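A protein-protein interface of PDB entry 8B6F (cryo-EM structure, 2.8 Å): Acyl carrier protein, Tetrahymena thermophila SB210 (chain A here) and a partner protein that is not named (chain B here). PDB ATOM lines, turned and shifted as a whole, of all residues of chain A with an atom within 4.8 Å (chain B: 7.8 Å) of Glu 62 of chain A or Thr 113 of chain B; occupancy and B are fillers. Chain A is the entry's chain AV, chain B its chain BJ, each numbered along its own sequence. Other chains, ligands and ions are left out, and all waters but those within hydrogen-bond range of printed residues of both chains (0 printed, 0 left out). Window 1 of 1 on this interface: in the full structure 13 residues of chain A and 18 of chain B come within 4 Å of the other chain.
The side-chain carboxylate (OE2) of Glu 59 of chain A is in salt-bridge range of the guanidinium group (NH2) of Arg 123 of chain B, at 3.0 Å. OE1 of Gln 61 of chain A lies close to OD1 of Asn 119 of chain B, 3.3 Å away. The backbone NH of Glu 62 of chain A sits close to the backbone carbonyl oxygen of Thr 113 of chain B (3.3 Å). SG of Cys 96 of chain B sits at hydrogen-bond distance from O of Ser 65 of chain A, at 3.4 Å.
NE2 of Gln 61 of chain A sits at hydrogen-bond distance from OE1 of Glu 59 of chain A (2.4 Å). NH1 of Arg 66 of chain A lies within salt-bridge range of OE2 of Glu 62 of chain A (3.7 Å). N of Gly 114 of chain B is in hydrogen-bond range of O of Pro 98 of chain B, at 3.1 Å. The side-chain amide nitrogen of Gln 112 of chain B is in hydrogen-bond range of the backbone carbonyl oxygen of Asn 116 of chain B (3.3 Å). OE1 of Gln 112 of chain B sits at hydrogen-bond distance from NE of Arg 123 of chain B. OD1 of Asn 116 of chain B lies close to OD1 of Asn 119 of chain B, at 2.6 Å.
Among the printed residues, pairs that only touch across the chains: Glu 59 of chain A with Asn 119 of chain B, Gln 61 of chain A with Thr 113 of chain B, Gln 61 of chain A with Gly 114 of chain B, Gln 61 of chain A with Gln 115 of chain B, Gln 61 of chain A with Asn 116 of chain B, Ser 65 of chain A with Gly 114 of chain B and Arg 66 of chain A with Cys 96 of chain B.
Glu 62 of chain A touches just one residue of chain B: Thr 113. Gln 61 of chain A touches just these residues of chain B: Thr 113, Gly 114, Gln 115, Asn 116 and Asn 119. Of the printed residues of chain A, Asn 116 of chain B touches Gln 61 (3.7 Å). Printed residues of chain A within 4 Å of Arg 123 of chain B: Glu 59 (3.0 Å). Printed residues of chain A within 4 Å of Cys 96 of chain B: Ser 65 (3.4 Å) and Arg 66 (3.9 Å). Leu 101 of chain B touches none of the printed residues of chain A. The nearest residue of chain A that does not touch Thr 113 of chain B is Ser 65 of chain A (4.3 Å).
Along chain B the printed residues that touch a printed residue of chain A span positions 96 to 123. Among the printed residues, 11 pairs touch across the chains. Among the printed residues, Asp or Glu carboxylates within 4 Å of a Lys or Arg side-chain nitrogen of the other chain: Glu 59 of chain A with Arg 123 of chain B (3.0 Å).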
ATOM      1  N   LEU A  58      -5.389  19.236  26.751  1.00  0.00           N
ATOM      2  CA  LEU A  58      -4.185  19.783  27.350  1.00  0.00           C
ATOM      3  C   LEU A  58      -3.315  18.657  27.903  1.00  0.00           C
ATOM      4  O   LEU A  58      -3.767  17.531  28.116  1.00  0.00           O
ATOM      5  CB  LEU A  58      -4.537  20.770  28.463  1.00  0.00           C
ATOM      6  CG  LEU A  58      -5.405  21.964  28.058  1.00  0.00           C
ATOM      7  CD1 LEU A  58      -5.646  22.870  29.252  1.00  0.00           C
ATOM      8  CD2 LEU A  58      -4.779  22.745  26.914  1.00  0.00           C
ATOM      9  N   GLU A  59      -2.049  18.979  28.135  1.00  0.00           N
ATOM     10  CA  GLU A  59      -1.070  18.018  28.612  1.00  0.00           C
ATOM     11  C   GLU A  59      -0.888  18.140  30.120  1.00  0.00           C
ATOM     12  O   GLU A  59      -1.195  19.166  30.730  1.00  0.00           O
ATOM     13  CB  GLU A  59       0.267  18.217  27.897  1.00  0.00           C
ATOM     14  CG  GLU A  59       0.198  17.910  26.409  1.00  0.00           C
ATOM     15  CD  GLU A  59       1.510  18.162  25.694  1.00  0.00           C
ATOM     16  OE1 GLU A  59       2.457  18.656  26.340  1.00  0.00           O
ATOM     17  OE2 GLU A  59       1.593  17.866  24.484  1.00  0.00           O
ATOM     18  N   LYS A  60      -0.370  17.066  30.716  1.00  0.00           N
ATOM     19  CA  LYS A  60      -0.291  16.987  32.171  1.00  0.00           C
ATOM     20  C   LYS A  60       0.598  18.084  32.743  1.00  0.00           C
ATOM     21  O   LYS A  60       0.238  18.727  33.735  1.00  0.00           O
ATOM     22  CB  LYS A  60       0.215  15.606  32.586  1.00  0.00           C
ATOM     23  CG  LYS A  60       0.113  15.327  34.077  1.00  0.00           C
ATOM     24  CD  LYS A  60       0.418  13.867  34.372  1.00  0.00           C
ATOM     25  CE  LYS A  60       0.271  13.547  35.847  1.00  0.00           C
ATOM     26  NZ  LYS A  60       1.269  14.270  36.679  1.00  0.00           N
ATOM     27  N   GLN A  61       1.763  18.319  32.135  1.00  0.00           N
ATOM     28  CA  GLN A  61       2.664  19.334  32.669  1.00  0.00           C
ATOM     29  C   GLN A  61       2.058  20.727  32.540  1.00  0.00           C
ATOM     30  O   GLN A  61       2.211  21.561  33.439  1.00  0.00           O
ATOM     31  CB  GLN A  61       4.028  19.263  31.974  1.00  0.00           C
ATOM     32  CG  GLN A  61       4.109  19.893  30.588  1.00  0.00           C
ATOM     33  CD  GLN A  61       3.293  19.157  29.556  1.00  0.00           C
ATOM     34  OE1 GLN A  61       2.864  18.028  29.779  1.00  0.00           O
ATOM     35  NE2 GLN A  61       3.071  19.795  28.414  1.00  0.00           N
ATOM     36  N   GLU A  62       1.374  21.002  31.427  1.00  0.00           N
ATOM     37  CA  GLU A  62       0.721  22.297  31.261  1.00  0.00           C
ATOM     38  C   GLU A  62      -0.356  22.507  32.317  1.00  0.00           C
ATOM     39  O   GLU A  62      -0.437  23.575  32.934  1.00  0.00           O
ATOM     40  CB  GLU A  62       0.127  22.405  29.857  1.00  0.00           C
ATOM     41  CG  GLU A  62      -0.797  23.598  29.671  1.00  0.00           C
ATOM     42  CD  GLU A  62      -1.214  23.790  28.227  1.00  0.00           C
ATOM     43  OE1 GLU A  62      -0.844  22.947  27.383  1.00  0.00           O
ATOM     44  OE2 GLU A  62      -1.911  24.785  27.936  1.00  0.00           O
ATOM     45  N   VAL A  63      -1.200  21.498  32.536  1.00  0.00           N
ATOM     46  CA  VAL A  63      -2.253  21.618  33.539  1.00  0.00           C
ATOM     47  C   VAL A  63      -1.651  21.838  34.920  1.00  0.00           C
ATOM     48  O   VAL A  63      -2.111  22.691  35.687  1.00  0.00           O
ATOM     49  CB  VAL A  63      -3.163  20.375  33.507  1.00  0.00           C
ATOM     50  CG1 VAL A  63      -4.133  20.377  34.683  1.00  0.00           C
ATOM     51  CG2 VAL A  63      -3.924  20.312  32.198  1.00  0.00           C
ATOM     52  N   GLU A  64      -0.609  21.076  35.260  1.00  0.00           N
ATOM     53  CA  GLU A  64       0.003  21.214  36.577  1.00  0.00           C
ATOM     54  C   GLU A  64       0.615  22.595  36.774  1.00  0.00           C
ATOM     55  O   GLU A  64       0.462  23.200  37.841  1.00  0.00           O
ATOM     56  CB  GLU A  64       1.063  20.128  36.764  1.00  0.00           C
ATOM     57  CG  GLU A  64       0.481  18.737  36.938  1.00  0.00           C
ATOM     58  CD  GLU A  64       1.543  17.686  37.172  1.00  0.00           C
ATOM     59  OE1 GLU A  64       2.738  17.995  36.989  1.00  0.00           O
ATOM     60  OE2 GLU A  64       1.183  16.551  37.546  1.00  0.00           O
ATOM     61  N   SER A  65       1.308  23.115  35.763  1.00  0.00           N
ATOM     62  CA  SER A  65       1.935  24.428  35.901  1.00  0.00           C
ATOM     63  C   SER A  65       0.900  25.536  36.019  1.00  0.00           C
ATOM     64  O   SER A  65       1.079  26.476  36.802  1.00  0.00           O
ATOM     65  CB  SER A  65       2.878  24.686  34.737  1.00  0.00           C
ATOM     66  OG  SER A  65       3.969  23.795  34.825  1.00  0.00           O
ATOM     67  N   ARG A  66      -0.182  25.456  35.245  1.00  0.00           N
ATOM     68  CA  ARG A  66      -1.222  26.471  35.357  1.00  0.00           C
ATOM     69  C   ARG A  66      -1.911  26.382  36.712  1.00  0.00           C
ATOM     70  O   ARG A  66      -2.255  27.410  37.305  1.00  0.00           O
ATOM     71  CB  ARG A  66      -2.224  26.319  34.213  1.00  0.00           C
ATOM     72  CG  ARG A  66      -1.604  26.557  32.840  1.00  0.00           C
ATOM     73  CD  ARG A  66      -2.591  26.312  31.712  1.00  0.00           C
ATOM     74  NE  ARG A  66      -3.613  27.347  31.645  1.00  0.00           N
ATOM     75  CZ  ARG A  66      -4.558  27.408  30.717  1.00  0.00           C
ATOM     76  NH1 ARG A  66      -4.638  26.508  29.752  1.00  0.00           N
ATOM     77  NH2 ARG A  66      -5.447  28.396  30.760  1.00  0.00           N
ATOM     78  N   ASN B  55       7.941  29.684  40.050  1.00  0.00           N
ATOM     79  CA  ASN B  55       7.607  28.289  39.793  1.00  0.00           C
ATOM     80  C   ASN B  55       8.778  27.397  40.187  1.00  0.00           C
ATOM     81  O   ASN B  55       9.878  27.567  39.643  1.00  0.00           O
ATOM     82  CB  ASN B  55       7.269  28.081  38.328  1.00  0.00           C
ATOM     83  CG  ASN B  55       6.650  26.723  38.061  1.00  0.00           C
ATOM     84  OD1 ASN B  55       6.911  25.757  38.775  1.00  0.00           O
ATOM     85  ND2 ASN B  55       5.821  26.645  37.029  1.00  0.00           N
ATOM     86  N   VAL B  94       3.819  35.704  27.289  1.00  0.00           N
ATOM     87  CA  VAL B  94       3.965  34.599  28.229  1.00  0.00           C
ATOM     88  C   VAL B  94       2.904  34.732  29.312  1.00  0.00           C
ATOM     89  O   VAL B  94       2.778  35.782  29.953  1.00  0.00           O
ATOM     90  CB  VAL B  94       5.377  34.586  28.834  1.00  0.00           C
ATOM     91  CG1 VAL B  94       5.556  33.385  29.754  1.00  0.00           C
ATOM     92  CG2 VAL B  94       6.426  34.590  27.737  1.00  0.00           C
ATOM     93  N   ARG B  95       2.131  33.665  29.516  1.00  0.00           N
ATOM     94  CA  ARG B  95       1.065  33.639  30.509  1.00  0.00           C
ATOM     95  C   ARG B  95       1.444  32.834  31.744  1.00  0.00           C
ATOM     96  O   ARG B  95       1.317  33.324  32.869  1.00  0.00           O
ATOM     97  CB  ARG B  95      -0.211  33.069  29.884  1.00  0.00           C
ATOM     98  CG  ARG B  95      -0.744  33.896  28.728  1.00  0.00           C
ATOM     99  CD  ARG B  95      -1.871  33.183  28.004  1.00  0.00           C
ATOM    100  NE  ARG B  95      -2.374  33.965  26.882  1.00  0.00           N
ATOM    101  CZ  ARG B  95      -3.315  33.552  26.043  1.00  0.00           C
ATOM    102  NH1 ARG B  95      -3.877  32.361  26.169  1.00  0.00           N
ATOM    103  NH2 ARG B  95      -3.702  34.353  25.056  1.00  0.00           N
ATOM    104  N   CYS B  96       1.908  31.605  31.551  1.00  0.00           N
ATOM    105  CA  CYS B  96       2.394  30.758  32.627  1.00  0.00           C
ATOM    106  C   CYS B  96       3.819  30.327  32.316  1.00  0.00           C
ATOM    107  O   CYS B  96       4.248  30.320  31.160  1.00  0.00           O
ATOM    108  CB  CYS B  96       1.495  29.530  32.816  1.00  0.00           C
ATOM    109  SG  CYS B  96       2.030  28.416  34.127  1.00  0.00           S
ATOM    110  N   GLU B  97       4.556  29.975  33.364  1.00  0.00           N
ATOM    111  CA  GLU B  97       5.959  29.627  33.229  1.00  0.00           C
ATOM    112  C   GLU B  97       6.244  28.319  33.950  1.00  0.00           C
ATOM    113  O   GLU B  97       5.570  27.987  34.929  1.00  0.00           O
ATOM    114  CB  GLU B  97       6.847  30.745  33.794  1.00  0.00           C
ATOM    115  CG  GLU B  97       6.374  32.133  33.383  1.00  0.00           C
ATOM    116  CD  GLU B  97       7.323  33.230  33.806  1.00  0.00           C
ATOM    117  OE1 GLU B  97       8.540  32.970  33.859  1.00  0.00           O
ATOM    118  OE2 GLU B  97       6.851  34.351  34.089  1.00  0.00           O
ATOM    119  N   PRO B  98       7.246  27.549  33.488  1.00  0.00           N
ATOM    120  CA  PRO B  98       8.173  27.852  32.391  1.00  0.00           C
ATOM    121  C   PRO B  98       7.510  27.748  31.028  1.00  0.00           C
ATOM    122  O   PRO B  98       6.604  26.948  30.823  1.00  0.00           O
ATOM    123  CB  PRO B  98       9.281  26.795  32.562  1.00  0.00           C
ATOM    124  CG  PRO B  98       8.876  25.910  33.731  1.00  0.00           C
ATOM    125  CD  PRO B  98       7.427  26.175  33.981  1.00  0.00           C
ATOM    126  N   GLU B  99       7.961  28.557  30.076  1.00  0.00           N
ATOM    127  CA  GLU B  99       7.351  28.655  28.760  1.00  0.00           C
ATOM    128  C   GLU B  99       8.396  28.332  27.704  1.00  0.00           C
ATOM    129  O   GLU B  99       9.512  28.858  27.755  1.00  0.00           O
ATOM    130  CB  GLU B  99       6.790  30.060  28.530  1.00  0.00           C
ATOM    131  CG  GLU B  99       5.704  30.151  27.477  1.00  0.00           C
ATOM    132  CD  GLU B  99       4.328  29.869  28.044  1.00  0.00           C
ATOM    133  OE1 GLU B  99       4.214  28.998  28.929  1.00  0.00           O
ATOM    134  OE2 GLU B  99       3.359  30.531  27.616  1.00  0.00           O
ATOM    135  N   PHE B 100       8.040  27.472  26.757  1.00  0.00           N
ATOM    136  CA  PHE B 100       8.893  27.156  25.621  1.00  0.00           C
ATOM    137  C   PHE B 100       8.180  27.603  24.356  1.00  0.00           C
ATOM    138  O   PHE B 100       7.003  27.284  24.160  1.00  0.00           O
ATOM    139  CB  PHE B 100       9.215  25.662  25.563  1.00  0.00           C
ATOM    140  CG  PHE B 100       9.920  25.146  26.781  1.00  0.00           C
ATOM    141  CD1 PHE B 100      11.301  25.169  26.857  1.00  0.00           C
ATOM    142  CD2 PHE B 100       9.203  24.638  27.850  1.00  0.00           C
ATOM    143  CE1 PHE B 100      11.954  24.693  27.977  1.00  0.00           C
ATOM    144  CE2 PHE B 100       9.850  24.159  28.972  1.00  0.00           C
ATOM    145  CZ  PHE B 100      11.228  24.188  29.036  1.00  0.00           C
ATOM    146  N   LEU B 101       8.888  28.336  23.504  1.00  0.00           N
ATOM    147  CA  LEU B 101       8.305  28.906  22.299  1.00  0.00           C
ATOM    148  C   LEU B 101       9.184  28.556  21.111  1.00  0.00           C
ATOM    149  O   LEU B 101      10.386  28.841  21.121  1.00  0.00           O
ATOM    150  CB  LEU B 101       8.158  30.425  22.438  1.00  0.00           C
ATOM    151  CG  LEU B 101       7.646  31.199  21.225  1.00  0.00           C
ATOM    152  CD1 LEU B 101       6.265  30.724  20.815  1.00  0.00           C
ATOM    153  CD2 LEU B 101       7.630  32.684  21.533  1.00  0.00           C
ATOM    154  N   ARG B 111       3.976  26.299  21.168  1.00  0.00           N
ATOM    155  CA  ARG B 111       4.293  26.787  22.499  1.00  0.00           C
ATOM    156  C   ARG B 111       3.932  25.713  23.512  1.00  0.00           C
ATOM    157  O   ARG B 111       2.891  25.062  23.394  1.00  0.00           O
ATOM    158  CB  ARG B 111       3.543  28.086  22.814  1.00  0.00           C
ATOM    159  CG  ARG B 111       4.097  28.840  24.007  1.00  0.00           C
ATOM    160  CD  ARG B 111       3.171  29.966  24.416  1.00  0.00           C
ATOM    161  NE  ARG B 111       3.048  30.993  23.388  1.00  0.00           N
ATOM    162  CZ  ARG B 111       3.746  32.121  23.360  1.00  0.00           C
ATOM    163  NH1 ARG B 111       4.646  32.403  24.287  1.00  0.00           N
ATOM    164  NH2 ARG B 111       3.530  32.993  22.379  1.00  0.00           N
ATOM    165  N   GLN B 112       4.799  25.532  24.501  1.00  0.00           N
ATOM    166  CA  GLN B 112       4.605  24.556  25.560  1.00  0.00           C
ATOM    167  C   GLN B 112       4.652  25.251  26.910  1.00  0.00           C
ATOM    168  O   GLN B 112       5.499  26.116  27.145  1.00  0.00           O
ATOM    169  CB  GLN B 112       5.668  23.456  25.510  1.00  0.00           C
ATOM    170  CG  GLN B 112       5.663  22.545  26.731  1.00  0.00           C
ATOM    171  CD  GLN B 112       6.556  21.339  26.563  1.00  0.00           C
ATOM    172  OE1 GLN B 112       6.850  20.922  25.447  1.00  0.00           O
ATOM    173  NE2 GLN B 112       6.993  20.767  27.679  1.00  0.00           N
ATOM    174  N   THR B 113       3.738  24.866  27.790  1.00  0.00           N
ATOM    175  CA  THR B 113       3.697  25.367  29.153  1.00  0.00           C
ATOM    176  C   THR B 113       3.982  24.206  30.089  1.00  0.00           C
ATOM    177  O   THR B 113       3.383  23.135  29.957  1.00  0.00           O
ATOM    178  CB  THR B 113       2.332  25.984  29.477  1.00  0.00           C
ATOM    179  OG1 THR B 113       2.048  27.047  28.559  1.00  0.00           O
ATOM    180  CG2 THR B 113       2.303  26.528  30.898  1.00  0.00           C
ATOM    181  N   GLY B 114       4.897  24.419  31.024  1.00  0.00           N
ATOM    182  CA  GLY B 114       5.292  23.400  31.969  1.00  0.00           C
ATOM    183  C   GLY B 114       6.529  22.641  31.530  1.00  0.00           C
ATOM    184  O   GLY B 114       6.960  22.685  30.376  1.00  0.00           O
ATOM    185  N   GLN B 115       7.099  21.924  32.493  1.00  0.00           N
ATOM    186  CA  GLN B 115       8.354  21.208  32.308  1.00  0.00           C
ATOM    187  C   GLN B 115       8.043  19.765  31.932  1.00  0.00           C
ATOM    188  O   GLN B 115       7.472  19.015  32.729  1.00  0.00           O
ATOM    189  CB  GLN B 115       9.197  21.277  33.580  1.00  0.00           C
ATOM    190  CG  GLN B 115      10.468  20.442  33.535  1.00  0.00           C
ATOM    191  CD  GLN B 115      10.240  18.996  33.928  1.00  0.00           C
ATOM    192  OE1 GLN B 115       9.402  18.696  34.775  1.00  0.00           O
ATOM    193  NE2 GLN B 115      10.985  18.092  33.306  1.00  0.00           N
ATOM    194  N   ASN B 116       8.418  19.383  30.712  1.00  0.00           N
ATOM    195  CA  ASN B 116       8.361  17.984  30.300  1.00  0.00           C
ATOM    196  C   ASN B 116       9.347  17.814  29.154  1.00  0.00           C
ATOM    197  O   ASN B 116       9.088  18.289  28.043  1.00  0.00           O
ATOM    198  CB  ASN B 116       6.953  17.585  29.888  1.00  0.00           C
ATOM    199  CG  ASN B 116       6.760  16.083  29.872  1.00  0.00           C
ATOM    200  OD1 ASN B 116       6.999  15.425  28.862  1.00  0.00           O
ATOM    201  ND2 ASN B 116       6.334  15.531  31.001  1.00  0.00           N
ATOM    202  N   ASN B 119       7.921  15.896  25.999  1.00  0.00           N
ATOM    203  CA  ASN B 119       7.006  16.685  25.182  1.00  0.00           C
ATOM    204  C   ASN B 119       7.738  17.808  24.457  1.00  0.00           C
ATOM    205  O   ASN B 119       7.434  18.106  23.298  1.00  0.00           O
ATOM    206  CB  ASN B 119       5.879  17.250  26.043  1.00  0.00           C
ATOM    207  CG  ASN B 119       4.970  16.168  26.590  1.00  0.00           C
ATOM    208  OD1 ASN B 119       4.719  16.101  27.791  1.00  0.00           O
ATOM    209  ND2 ASN B 119       4.468  15.314  25.706  1.00  0.00           N
ATOM    210  N   ARG B 123       7.866  18.223  20.419  1.00  0.00           N
ATOM    211  CA  ARG B 123       7.497  19.438  19.701  1.00  0.00           C
ATOM    212  C   ARG B 123       8.625  19.894  18.787  1.00  0.00           C
ATOM    213  O   ARG B 123       8.382  20.304  17.647  1.00  0.00           O
ATOM    214  CB  ARG B 123       7.129  20.541  20.691  1.00  0.00           C
ATOM    215  CG  ARG B 123       5.855  20.263  21.464  1.00  0.00           C
ATOM    216  CD  ARG B 123       5.547  21.378  22.447  1.00  0.00           C
ATOM    217  NE  ARG B 123       4.491  20.995  23.377  1.00  0.00           N
ATOM    218  CZ  ARG B 123       3.192  21.088  23.125  1.00  0.00           C
ATOM    219  NH1 ARG B 123       2.742  21.543  21.968  1.00  0.00           N
ATOM    220  NH2 ARG B 123       2.323  20.713  24.058  1.00  0.00           N
